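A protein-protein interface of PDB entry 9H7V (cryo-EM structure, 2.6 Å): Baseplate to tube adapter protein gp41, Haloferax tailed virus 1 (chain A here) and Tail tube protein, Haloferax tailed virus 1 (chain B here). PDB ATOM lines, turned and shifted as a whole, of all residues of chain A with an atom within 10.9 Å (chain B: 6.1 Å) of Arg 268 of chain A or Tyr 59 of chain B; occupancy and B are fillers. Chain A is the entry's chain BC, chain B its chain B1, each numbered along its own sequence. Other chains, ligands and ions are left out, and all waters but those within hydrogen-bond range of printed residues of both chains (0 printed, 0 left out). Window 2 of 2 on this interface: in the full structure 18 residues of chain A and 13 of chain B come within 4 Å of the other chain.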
ATOM      1  N   GLY A 170      -6.887  -6.920 -10.780  1.00  0.00           N
ATOM      2  CA  GLY A 170      -5.635  -6.454 -11.353  1.00  0.00           C
ATOM      3  C   GLY A 170      -4.420  -7.208 -10.817  1.00  0.00           C
ATOM      4  O   GLY A 170      -3.295  -6.742 -10.992  1.00  0.00           O
ATOM      5  N   PHE A 210      -1.617  -5.086  -7.474  1.00  0.00           N
ATOM      6  CA  PHE A 210      -3.066  -5.224  -7.425  1.00  0.00           C
ATOM      7  C   PHE A 210      -3.744  -3.873  -7.219  1.00  0.00           C
ATOM      8  O   PHE A 210      -3.093  -2.881  -6.898  1.00  0.00           O
ATOM      9  CB  PHE A 210      -3.499  -6.236  -6.357  1.00  0.00           C
ATOM     10  CG  PHE A 210      -3.058  -5.950  -4.943  1.00  0.00           C
ATOM     11  CD1 PHE A 210      -3.826  -5.156  -4.100  1.00  0.00           C
ATOM     12  CD2 PHE A 210      -1.888  -6.506  -4.441  1.00  0.00           C
ATOM     13  CE1 PHE A 210      -3.424  -4.910  -2.794  1.00  0.00           C
ATOM     14  CE2 PHE A 210      -1.485  -6.256  -3.136  1.00  0.00           C
ATOM     15  CZ  PHE A 210      -2.254  -5.459  -2.316  1.00  0.00           C
ATOM     16  N   GLU A 211      -5.070  -3.868  -7.409  1.00  0.00           N
ATOM     17  CA  GLU A 211      -5.893  -2.688  -7.202  1.00  0.00           C
ATOM     18  C   GLU A 211      -6.962  -3.009  -6.157  1.00  0.00           C
ATOM     19  O   GLU A 211      -7.732  -3.953  -6.319  1.00  0.00           O
ATOM     20  CB  GLU A 211      -6.403  -2.150  -8.544  1.00  0.00           C
ATOM     21  CG  GLU A 211      -5.274  -1.938  -9.548  1.00  0.00           C
ATOM     22  CD  GLU A 211      -5.467  -0.982 -10.714  1.00  0.00           C
ATOM     23  OE1 GLU A 211      -6.337  -0.100 -10.631  1.00  0.00           O
ATOM     24  OE2 GLU A 211      -4.729  -1.124 -11.711  1.00  0.00           O
ATOM     25  N   THR A 212      -6.960  -2.224  -5.070  1.00  0.00           N
ATOM     26  CA  THR A 212      -7.858  -2.409  -3.939  1.00  0.00           C
ATOM     27  C   THR A 212      -9.148  -1.643  -4.210  1.00  0.00           C
ATOM     28  O   THR A 212      -9.147  -0.413  -4.225  1.00  0.00           O
ATOM     29  CB  THR A 212      -7.196  -1.966  -2.625  1.00  0.00           C
ATOM     30  OG1 THR A 212      -5.855  -2.455  -2.578  1.00  0.00           O
ATOM     31  CG2 THR A 212      -7.944  -2.430  -1.394  1.00  0.00           C
ATOM     32  N   LEU A 213     -10.246  -2.383  -4.413  1.00  0.00           N
ATOM     33  CA  LEU A 213     -11.460  -1.800  -4.965  1.00  0.00           C
ATOM     34  C   LEU A 213     -12.517  -1.564  -3.890  1.00  0.00           C
ATOM     35  O   LEU A 213     -13.210  -0.549  -3.933  1.00  0.00           O
ATOM     36  CB  LEU A 213     -11.998  -2.682  -6.097  1.00  0.00           C
ATOM     37  CG  LEU A 213     -11.130  -2.803  -7.351  1.00  0.00           C
ATOM     38  CD1 LEU A 213     -11.886  -3.552  -8.433  1.00  0.00           C
ATOM     39  CD2 LEU A 213     -10.693  -1.441  -7.873  1.00  0.00           C
ATOM     40  N   ILE A 216     -11.672  -0.725   1.323  1.00  0.00           N
ATOM     41  CA  ILE A 216     -10.347  -0.177   1.062  1.00  0.00           C
ATOM     42  C   ILE A 216      -9.614   0.122   2.372  1.00  0.00           C
ATOM     43  O   ILE A 216      -8.500  -0.371   2.544  1.00  0.00           O
ATOM     44  CB  ILE A 216     -10.401   1.020   0.082  1.00  0.00           C
ATOM     45  CG1 ILE A 216     -10.621   0.553  -1.359  1.00  0.00           C
ATOM     46  CG2 ILE A 216      -9.162   1.899   0.200  1.00  0.00           C
ATOM     47  CD1 ILE A 216     -11.193   1.610  -2.279  1.00  0.00           C
ATOM     48  N   VAL A 263      -0.871   3.981  -3.888  1.00  0.00           N
ATOM     49  CA  VAL A 263      -0.928   5.041  -4.886  1.00  0.00           C
ATOM     50  C   VAL A 263      -2.378   5.478  -5.091  1.00  0.00           C
ATOM     51  O   VAL A 263      -3.255   4.657  -5.359  1.00  0.00           O
ATOM     52  CB  VAL A 263      -0.219   4.653  -6.201  1.00  0.00           C
ATOM     53  CG1 VAL A 263      -0.616   5.538  -7.376  1.00  0.00           C
ATOM     54  CG2 VAL A 263       1.292   4.663  -6.036  1.00  0.00           C
ATOM     55  N   HIS A 264      -2.589   6.791  -4.950  1.00  0.00           N
ATOM     56  CA  HIS A 264      -3.859   7.463  -5.166  1.00  0.00           C
ATOM     57  C   HIS A 264      -3.743   8.347  -6.405  1.00  0.00           C
ATOM     58  O   HIS A 264      -2.818   9.151  -6.505  1.00  0.00           O
ATOM     59  CB  HIS A 264      -4.208   8.315  -3.940  1.00  0.00           C
ATOM     60  CG  HIS A 264      -4.546   7.533  -2.717  1.00  0.00           C
ATOM     61  ND1 HIS A 264      -3.590   6.888  -1.957  1.00  0.00           N
ATOM     62  CD2 HIS A 264      -5.730   7.306  -2.111  1.00  0.00           C
ATOM     63  CE1 HIS A 264      -4.174   6.288  -0.941  1.00  0.00           C
ATOM     64  NE2 HIS A 264      -5.484   6.531  -1.012  1.00  0.00           N
ATOM     65  N   GLN A 265      -4.691   8.191  -7.337  1.00  0.00           N
ATOM     66  CA  GLN A 265      -4.682   8.938  -8.585  1.00  0.00           C
ATOM     67  C   GLN A 265      -5.922   9.824  -8.669  1.00  0.00           C
ATOM     68  O   GLN A 265      -6.974   9.470  -8.137  1.00  0.00           O
ATOM     69  CB  GLN A 265      -4.575   7.990  -9.779  1.00  0.00           C
ATOM     70  CG  GLN A 265      -3.159   7.490 -10.024  1.00  0.00           C
ATOM     71  CD  GLN A 265      -3.120   6.380 -11.046  1.00  0.00           C
ATOM     72  OE1 GLN A 265      -3.313   5.210 -10.727  1.00  0.00           O
ATOM     73  NE2 GLN A 265      -2.859   6.745 -12.290  1.00  0.00           N
ATOM     74  N   ALA A 266      -5.768  10.970  -9.344  1.00  0.00           N
ATOM     75  CA  ALA A 266      -6.815  11.970  -9.491  1.00  0.00           C
ATOM     76  C   ALA A 266      -8.013  11.376 -10.224  1.00  0.00           C
ATOM     77  O   ALA A 266      -7.861  10.778 -11.289  1.00  0.00           O
ATOM     78  CB  ALA A 266      -6.268  13.180 -10.211  1.00  0.00           C
ATOM     79  N   GLY A 267      -9.197  11.515  -9.617  1.00  0.00           N
ATOM     80  CA  GLY A 267     -10.452  11.147 -10.252  1.00  0.00           C
ATOM     81  C   GLY A 267     -10.796   9.662 -10.143  1.00  0.00           C
ATOM     82  O   GLY A 267     -11.762   9.221 -10.762  1.00  0.00           O
ATOM     83  N   ARG A 268     -10.022   8.903  -9.354  1.00  0.00           N
ATOM     84  CA  ARG A 268     -10.253   7.476  -9.167  1.00  0.00           C
ATOM     85  C   ARG A 268     -10.673   7.210  -7.724  1.00  0.00           C
ATOM     86  O   ARG A 268     -10.104   7.785  -6.798  1.00  0.00           O
ATOM     87  CB  ARG A 268      -9.000   6.660  -9.500  1.00  0.00           C
ATOM     88  CG  ARG A 268      -8.442   6.909 -10.893  1.00  0.00           C
ATOM     89  CD  ARG A 268      -7.466   5.840 -11.336  1.00  0.00           C
ATOM     90  NE  ARG A 268      -6.918   6.185 -12.641  1.00  0.00           N
ATOM     91  CZ  ARG A 268      -6.243   5.365 -13.439  1.00  0.00           C
ATOM     92  NH1 ARG A 268      -5.797   5.806 -14.602  1.00  0.00           N
ATOM     93  NH2 ARG A 268      -6.016   4.111 -13.084  1.00  0.00           N
ATOM     94  N   GLY A 269     -11.645   6.307  -7.548  1.00  0.00           N
ATOM     95  CA  GLY A 269     -12.215   6.025  -6.240  1.00  0.00           C
ATOM     96  C   GLY A 269     -11.560   4.842  -5.529  1.00  0.00           C
ATOM     97  O   GLY A 269     -12.141   4.303  -4.590  1.00  0.00           O
ATOM     98  N   TRP A 270     -10.350   4.458  -5.964  1.00  0.00           N
ATOM     99  CA  TRP A 270      -9.696   3.256  -5.464  1.00  0.00           C
ATOM    100  C   TRP A 270      -8.190   3.469  -5.296  1.00  0.00           C
ATOM    101  O   TRP A 270      -7.648   4.465  -5.772  1.00  0.00           O
ATOM    102  CB  TRP A 270     -10.038   2.053  -6.357  1.00  0.00           C
ATOM    103  CG  TRP A 270      -9.385   2.043  -7.706  1.00  0.00           C
ATOM    104  CD1 TRP A 270      -8.134   1.584  -8.000  1.00  0.00           C
ATOM    105  CD2 TRP A 270      -9.957   2.471  -8.958  1.00  0.00           C
ATOM    106  NE1 TRP A 270      -7.878   1.716  -9.336  1.00  0.00           N
ATOM    107  CE2 TRP A 270      -8.977   2.251  -9.953  1.00  0.00           C
ATOM    108  CE3 TRP A 270     -11.188   3.022  -9.339  1.00  0.00           C
ATOM    109  CZ2 TRP A 270      -9.190   2.564 -11.296  1.00  0.00           C
ATOM    110  CZ3 TRP A 270     -11.397   3.333 -10.666  1.00  0.00           C
ATOM    111  CH2 TRP A 270     -10.411   3.105 -11.630  1.00  0.00           C
ATOM    112  N   VAL A 271      -7.530   2.519  -4.615  1.00  0.00           N
ATOM    113  CA  VAL A 271      -6.102   2.588  -4.330  1.00  0.00           C
ATOM    114  C   VAL A 271      -5.371   1.528  -5.152  1.00  0.00           C
ATOM    115  O   VAL A 271      -5.796   0.375  -5.212  1.00  0.00           O
ATOM    116  CB  VAL A 271      -5.801   2.460  -2.821  1.00  0.00           C
ATOM    117  CG1 VAL A 271      -4.320   2.620  -2.508  1.00  0.00           C
ATOM    118  CG2 VAL A 271      -6.611   3.449  -1.998  1.00  0.00           C
ATOM    119  N   THR A 272      -4.264   1.950  -5.776  1.00  0.00           N
ATOM    120  CA  THR A 272      -3.377   1.078  -6.529  1.00  0.00           C
ATOM    121  C   THR A 272      -2.187   0.698  -5.652  1.00  0.00           C
ATOM    122  O   THR A 272      -1.580   1.557  -5.016  1.00  0.00           O
ATOM    123  CB  THR A 272      -2.925   1.752  -7.832  1.00  0.00           C
ATOM    124  OG1 THR A 272      -4.088   2.124  -8.572  1.00  0.00           O
ATOM    125  CG2 THR A 272      -2.049   0.874  -8.700  1.00  0.00           C
ATOM    126  N   VAL A 273      -1.881  -0.604  -5.625  1.00  0.00           N
ATOM    127  CA  VAL A 273      -0.639  -1.107  -5.063  1.00  0.00           C
ATOM    128  C   VAL A 273       0.261  -1.505  -6.233  1.00  0.00           C
ATOM    129  O   VAL A 273       0.068  -2.567  -6.825  1.00  0.00           O
ATOM    130  CB  VAL A 273      -0.888  -2.256  -4.063  1.00  0.00           C
ATOM    131  CG1 VAL A 273       0.403  -2.909  -3.589  1.00  0.00           C
ATOM    132  CG2 VAL A 273      -1.708  -1.788  -2.870  1.00  0.00           C
ATOM    133  N   PRO A 274       1.230  -0.644  -6.639  1.00  0.00           N
ATOM    134  CA  PRO A 274       2.143  -0.963  -7.739  1.00  0.00           C
ATOM    135  C   PRO A 274       3.047  -2.150  -7.412  1.00  0.00           C
ATOM    136  O   PRO A 274       3.265  -3.009  -8.264  1.00  0.00           O
ATOM    137  CB  PRO A 274       2.989   0.307  -7.917  1.00  0.00           C
ATOM    138  CG  PRO A 274       2.181   1.390  -7.246  1.00  0.00           C
ATOM    139  CD  PRO A 274       1.483   0.699  -6.095  1.00  0.00           C
ATOM    140  N   ALA B  39     -19.931  10.888 -19.438  1.00  0.00           N
ATOM    141  CA  ALA B  39     -18.881   9.933 -19.748  1.00  0.00           C
ATOM    142  C   ALA B  39     -18.015   9.692 -18.516  1.00  0.00           C
ATOM    143  O   ALA B  39     -17.657  10.632 -17.806  1.00  0.00           O
ATOM    144  CB  ALA B  39     -18.050  10.453 -20.895  1.00  0.00           C
ATOM    145  N   TYR B  40     -17.703   8.415 -18.279  1.00  0.00           N
ATOM    146  CA  TYR B  40     -16.661   8.012 -17.350  1.00  0.00           C
ATOM    147  C   TYR B  40     -15.605   7.230 -18.124  1.00  0.00           C
ATOM    148  O   TYR B  40     -15.906   6.608 -19.142  1.00  0.00           O
ATOM    149  CB  TYR B  40     -17.213   7.081 -16.267  1.00  0.00           C
ATOM    150  CG  TYR B  40     -18.295   7.611 -15.356  1.00  0.00           C
ATOM    151  CD1 TYR B  40     -19.630   7.571 -15.734  1.00  0.00           C
ATOM    152  CD2 TYR B  40     -17.997   8.074 -14.083  1.00  0.00           C
ATOM    153  CE1 TYR B  40     -20.634   8.018 -14.889  1.00  0.00           C
ATOM    154  CE2 TYR B  40     -18.989   8.522 -13.223  1.00  0.00           C
ATOM    155  CZ  TYR B  40     -20.312   8.495 -13.630  1.00  0.00           C
ATOM    156  OH  TYR B  40     -21.296   8.940 -12.795  1.00  0.00           O
ATOM    157  N   GLU B  41     -14.366   7.273 -17.623  1.00  0.00           N
ATOM    158  CA  GLU B  41     -13.322   6.357 -18.046  1.00  0.00           C
ATOM    159  C   GLU B  41     -13.551   5.021 -17.342  1.00  0.00           C
ATOM    160  O   GLU B  41     -13.915   4.999 -16.168  1.00  0.00           O
ATOM    161  CB  GLU B  41     -11.948   6.924 -17.690  1.00  0.00           C
ATOM    162  CG  GLU B  41     -11.562   8.178 -18.456  1.00  0.00           C
ATOM    163  CD  GLU B  41     -11.204   8.008 -19.925  1.00  0.00           C
ATOM    164  OE1 GLU B  41     -11.014   6.856 -20.371  1.00  0.00           O
ATOM    165  OE2 GLU B  41     -11.112   9.036 -20.625  1.00  0.00           O
ATOM    166  N   HIS B  42     -13.346   3.917 -18.074  1.00  0.00           N
ATOM    167  CA  HIS B  42     -13.513   2.579 -17.529  1.00  0.00           C
ATOM    168  C   HIS B  42     -12.160   1.889 -17.393  1.00  0.00           C
ATOM    169  O   HIS B  42     -11.415   1.781 -18.367  1.00  0.00           O
ATOM    170  CB  HIS B  42     -14.493   1.757 -18.379  1.00  0.00           C
ATOM    171  CG  HIS B  42     -15.931   2.015 -18.074  1.00  0.00           C
ATOM    172  ND1 HIS B  42     -16.939   1.182 -18.512  1.00  0.00           N
ATOM    173  CD2 HIS B  42     -16.534   2.998 -17.371  1.00  0.00           C
ATOM    174  CE1 HIS B  42     -18.102   1.646 -18.100  1.00  0.00           C
ATOM    175  NE2 HIS B  42     -17.879   2.759 -17.397  1.00  0.00           N
ATOM    176  N   ALA B  43     -11.865   1.433 -16.171  1.00  0.00           N
ATOM    177  CA  ALA B  43     -10.733   0.558 -15.915  1.00  0.00           C
ATOM    178  C   ALA B  43     -11.225  -0.884 -15.852  1.00  0.00           C
ATOM    179  O   ALA B  43     -11.999  -1.238 -14.964  1.00  0.00           O
ATOM    180  CB  ALA B  43     -10.033   0.971 -14.643  1.00  0.00           C
ATOM    181  N   LYS B  57     -14.466  -0.611 -13.400  1.00  0.00           N
ATOM    182  CA  LYS B  57     -14.666   0.519 -12.507  1.00  0.00           C
ATOM    183  C   LYS B  57     -14.696   1.829 -13.294  1.00  0.00           C
ATOM    184  O   LYS B  57     -14.017   1.962 -14.310  1.00  0.00           O
ATOM    185  CB  LYS B  57     -13.576   0.548 -11.428  1.00  0.00           C
ATOM    186  CG  LYS B  57     -13.688  -0.504 -10.331  1.00  0.00           C
ATOM    187  CD  LYS B  57     -14.820  -0.255  -9.354  1.00  0.00           C
ATOM    188  CE  LYS B  57     -14.834  -1.211  -8.182  1.00  0.00           C
ATOM    189  NZ  LYS B  57     -15.752  -0.752  -7.114  1.00  0.00           N
ATOM    190  N   ARG B  58     -15.486   2.787 -12.788  1.00  0.00           N
ATOM    191  CA  ARG B  58     -15.649   4.117 -13.357  1.00  0.00           C
ATOM    192  C   ARG B  58     -14.657   5.079 -12.709  1.00  0.00           C
ATOM    193  O   ARG B  58     -14.454   5.034 -11.496  1.00  0.00           O
ATOM    194  CB  ARG B  58     -17.051   4.666 -13.067  1.00  0.00           C
ATOM    195  CG  ARG B  58     -18.200   3.839 -13.625  1.00  0.00           C
ATOM    196  CD  ARG B  58     -19.514   4.594 -13.704  1.00  0.00           C
ATOM    197  NE  ARG B  58     -20.174   4.860 -12.430  1.00  0.00           N
ATOM    198  CZ  ARG B  58     -21.477   5.094 -12.281  1.00  0.00           C
ATOM    199  NH1 ARG B  58     -21.971   5.327 -11.078  1.00  0.00           N
ATOM    200  NH2 ARG B  58     -22.285   5.085 -13.327  1.00  0.00           N
ATOM    201  N   TYR B  59     -14.057   5.954 -13.529  1.00  0.00           N
ATOM    202  CA  TYR B  59     -13.232   7.055 -13.048  1.00  0.00           C
ATOM    203  C   TYR B  59     -13.397   8.283 -13.943  1.00  0.00           C
ATOM    204  O   TYR B  59     -13.878   8.167 -15.070  1.00  0.00           O
ATOM    205  CB  TYR B  59     -11.781   6.616 -12.807  1.00  0.00           C
ATOM    206  CG  TYR B  59     -10.923   6.257 -13.999  1.00  0.00           C
ATOM    207  CD1 TYR B  59     -10.992   5.000 -14.582  1.00  0.00           C
ATOM    208  CD2 TYR B  59      -9.973   7.144 -14.494  1.00  0.00           C
ATOM    209  CE1 TYR B  59     -10.179   4.647 -15.649  1.00  0.00           C
ATOM    210  CE2 TYR B  59      -9.151   6.807 -15.561  1.00  0.00           C
ATOM    211  CZ  TYR B  59      -9.254   5.553 -16.142  1.00  0.00           C
ATOM    212  OH  TYR B  59      -8.457   5.214 -17.197  1.00  0.00           O
ATOM    213  N   GLU B  60     -13.024   9.454 -13.398  1.00  0.00           N
ATOM    214  CA  GLU B  60     -12.819  10.698 -14.129  1.00  0.00           C
ATOM    215  C   GLU B  60     -14.084  11.074 -14.906  1.00  0.00           C
ATOM    216  O   GLU B  60     -14.112  10.995 -16.134  1.00  0.00           O
ATOM    217  CB  GLU B  60     -11.567  10.572 -15.007  1.00  0.00           C
ATOM    218  CG  GLU B  60     -10.984  11.891 -15.488  1.00  0.00           C
ATOM    219  CD  GLU B  60      -9.832  11.748 -16.471  1.00  0.00           C
ATOM    220  OE1 GLU B  60      -8.951  10.895 -16.237  1.00  0.00           O
ATOM    221  OE2 GLU B  60      -9.819  12.493 -17.471  1.00  0.00           O
ATOM    222  N   HIS B  61     -15.124  11.479 -14.167  1.00  0.00           N
ATOM    223  CA  HIS B  61     -16.426  11.791 -14.735  1.00  0.00           C
ATOM    224  C   HIS B  61     -16.376  13.106 -15.509  1.00  0.00           C
ATOM    225  O   HIS B  61     -15.668  14.036 -15.129  1.00  0.00           O
ATOM    226  CB  HIS B  61     -17.512  11.790 -13.650  1.00  0.00           C
ATOM    227  CG  HIS B  61     -18.890  12.006 -14.178  1.00  0.00           C
ATOM    228  ND1 HIS B  61     -19.436  11.215 -15.172  1.00  0.00           N
ATOM    229  CD2 HIS B  61     -19.832  12.918 -13.862  1.00  0.00           C
ATOM    230  CE1 HIS B  61     -20.656  11.630 -15.441  1.00  0.00           C
ATOM    231  NE2 HIS B  61     -20.922  12.674 -14.651  1.00  0.00           N
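The backbone NH (N) of Glu 60 of chain B lies within hydrogen-bond range of the backbone carbonyl oxygen (O) of Gly 267 of chain A (2.9 Å).
The backbone NH of Glu 41 of chain B sits at hydrogen-bond distance from the backbone carbonyl oxygen of Tyr 59 of chain B. The backbone carbonyl oxygen (O) of Lys 57 of chain B sits at hydrogen-bond distance from the backbone NH (N) of Ala 43 of chain B (2.9 Å). The side-chain carboxylate of Glu 211 of chain A lies within hydrogen-bond range of the indole nitrogen of Trp 270 of chain A (2.7 Å).
Among the printed residues, merely in contact across the chains: Leu 213 of chain A with Lys 57 of chain B, Gly 267 of chain A with Tyr 59 of chain B, Arg 268 of chain A with Tyr 59 of chain B, Trp 270 of chain A with Ala 43 of chain B, Trp 270 of chain A with Lys 57 of chain B, Trp 270 of chain A with Arg 58 of chain B and Trp 270 of chain A with Tyr 59 of chain B.
Of chain A, only Gly 267, Arg 268 and Trp 270 come within 4 Å of Tyr 59 of chain B. No residue of chain A comes within 4 Å of Glu 41 of chain B. Printed residues of chain A within 4 Å of Ala 43 of chain B: Trp 270 (3.7 Å). Of the printed residues of chain B, Leu 213 of chain A touches Lys 57 (3.8 Å). Of the printed residues of chain A, Lys 57 of chain B touches Leu 213 and Trp 270. Of the printed residues of chain B, Gly 267 of chain A touches Tyr 59 and Glu 60. Pro 274 of chain A touches none of the printed residues of chain B. Gly 170 of chain A touches none of the printed residues of chain B. The nearest printed residue of chain A that does not touch Tyr 59 of chain B is Gly 269 of chain A (5.3 Å). The nearest printed residue of chain B that does not touch Gly 267 of chain A is Arg 58 of chain B (5.0 Å).
Of the 10 printed residues of chain B, 5 touch a printed residue of chain A. Hydrophobic or aromatic side chains of chain B within 4 Å of the printed part of chain A: Ala 43 and Tyr 59. Along chain B the printed residues that touch a printed residue of chain A span positions 43 to 60. Of the 18 printed residues of chain A, 4 touch a printed residue of chain B. Hydrophobic or aromatic side chains of chain A within 4 Å of the printed part of chain B: Leu 213 and Trp 270. Among the printed residues, 8 pairs touch across the chains. Among the printed residues, no Asp or Glu carboxylate lies within 4 Å of a Lys or Arg side-chain nitrogen of the other chain.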
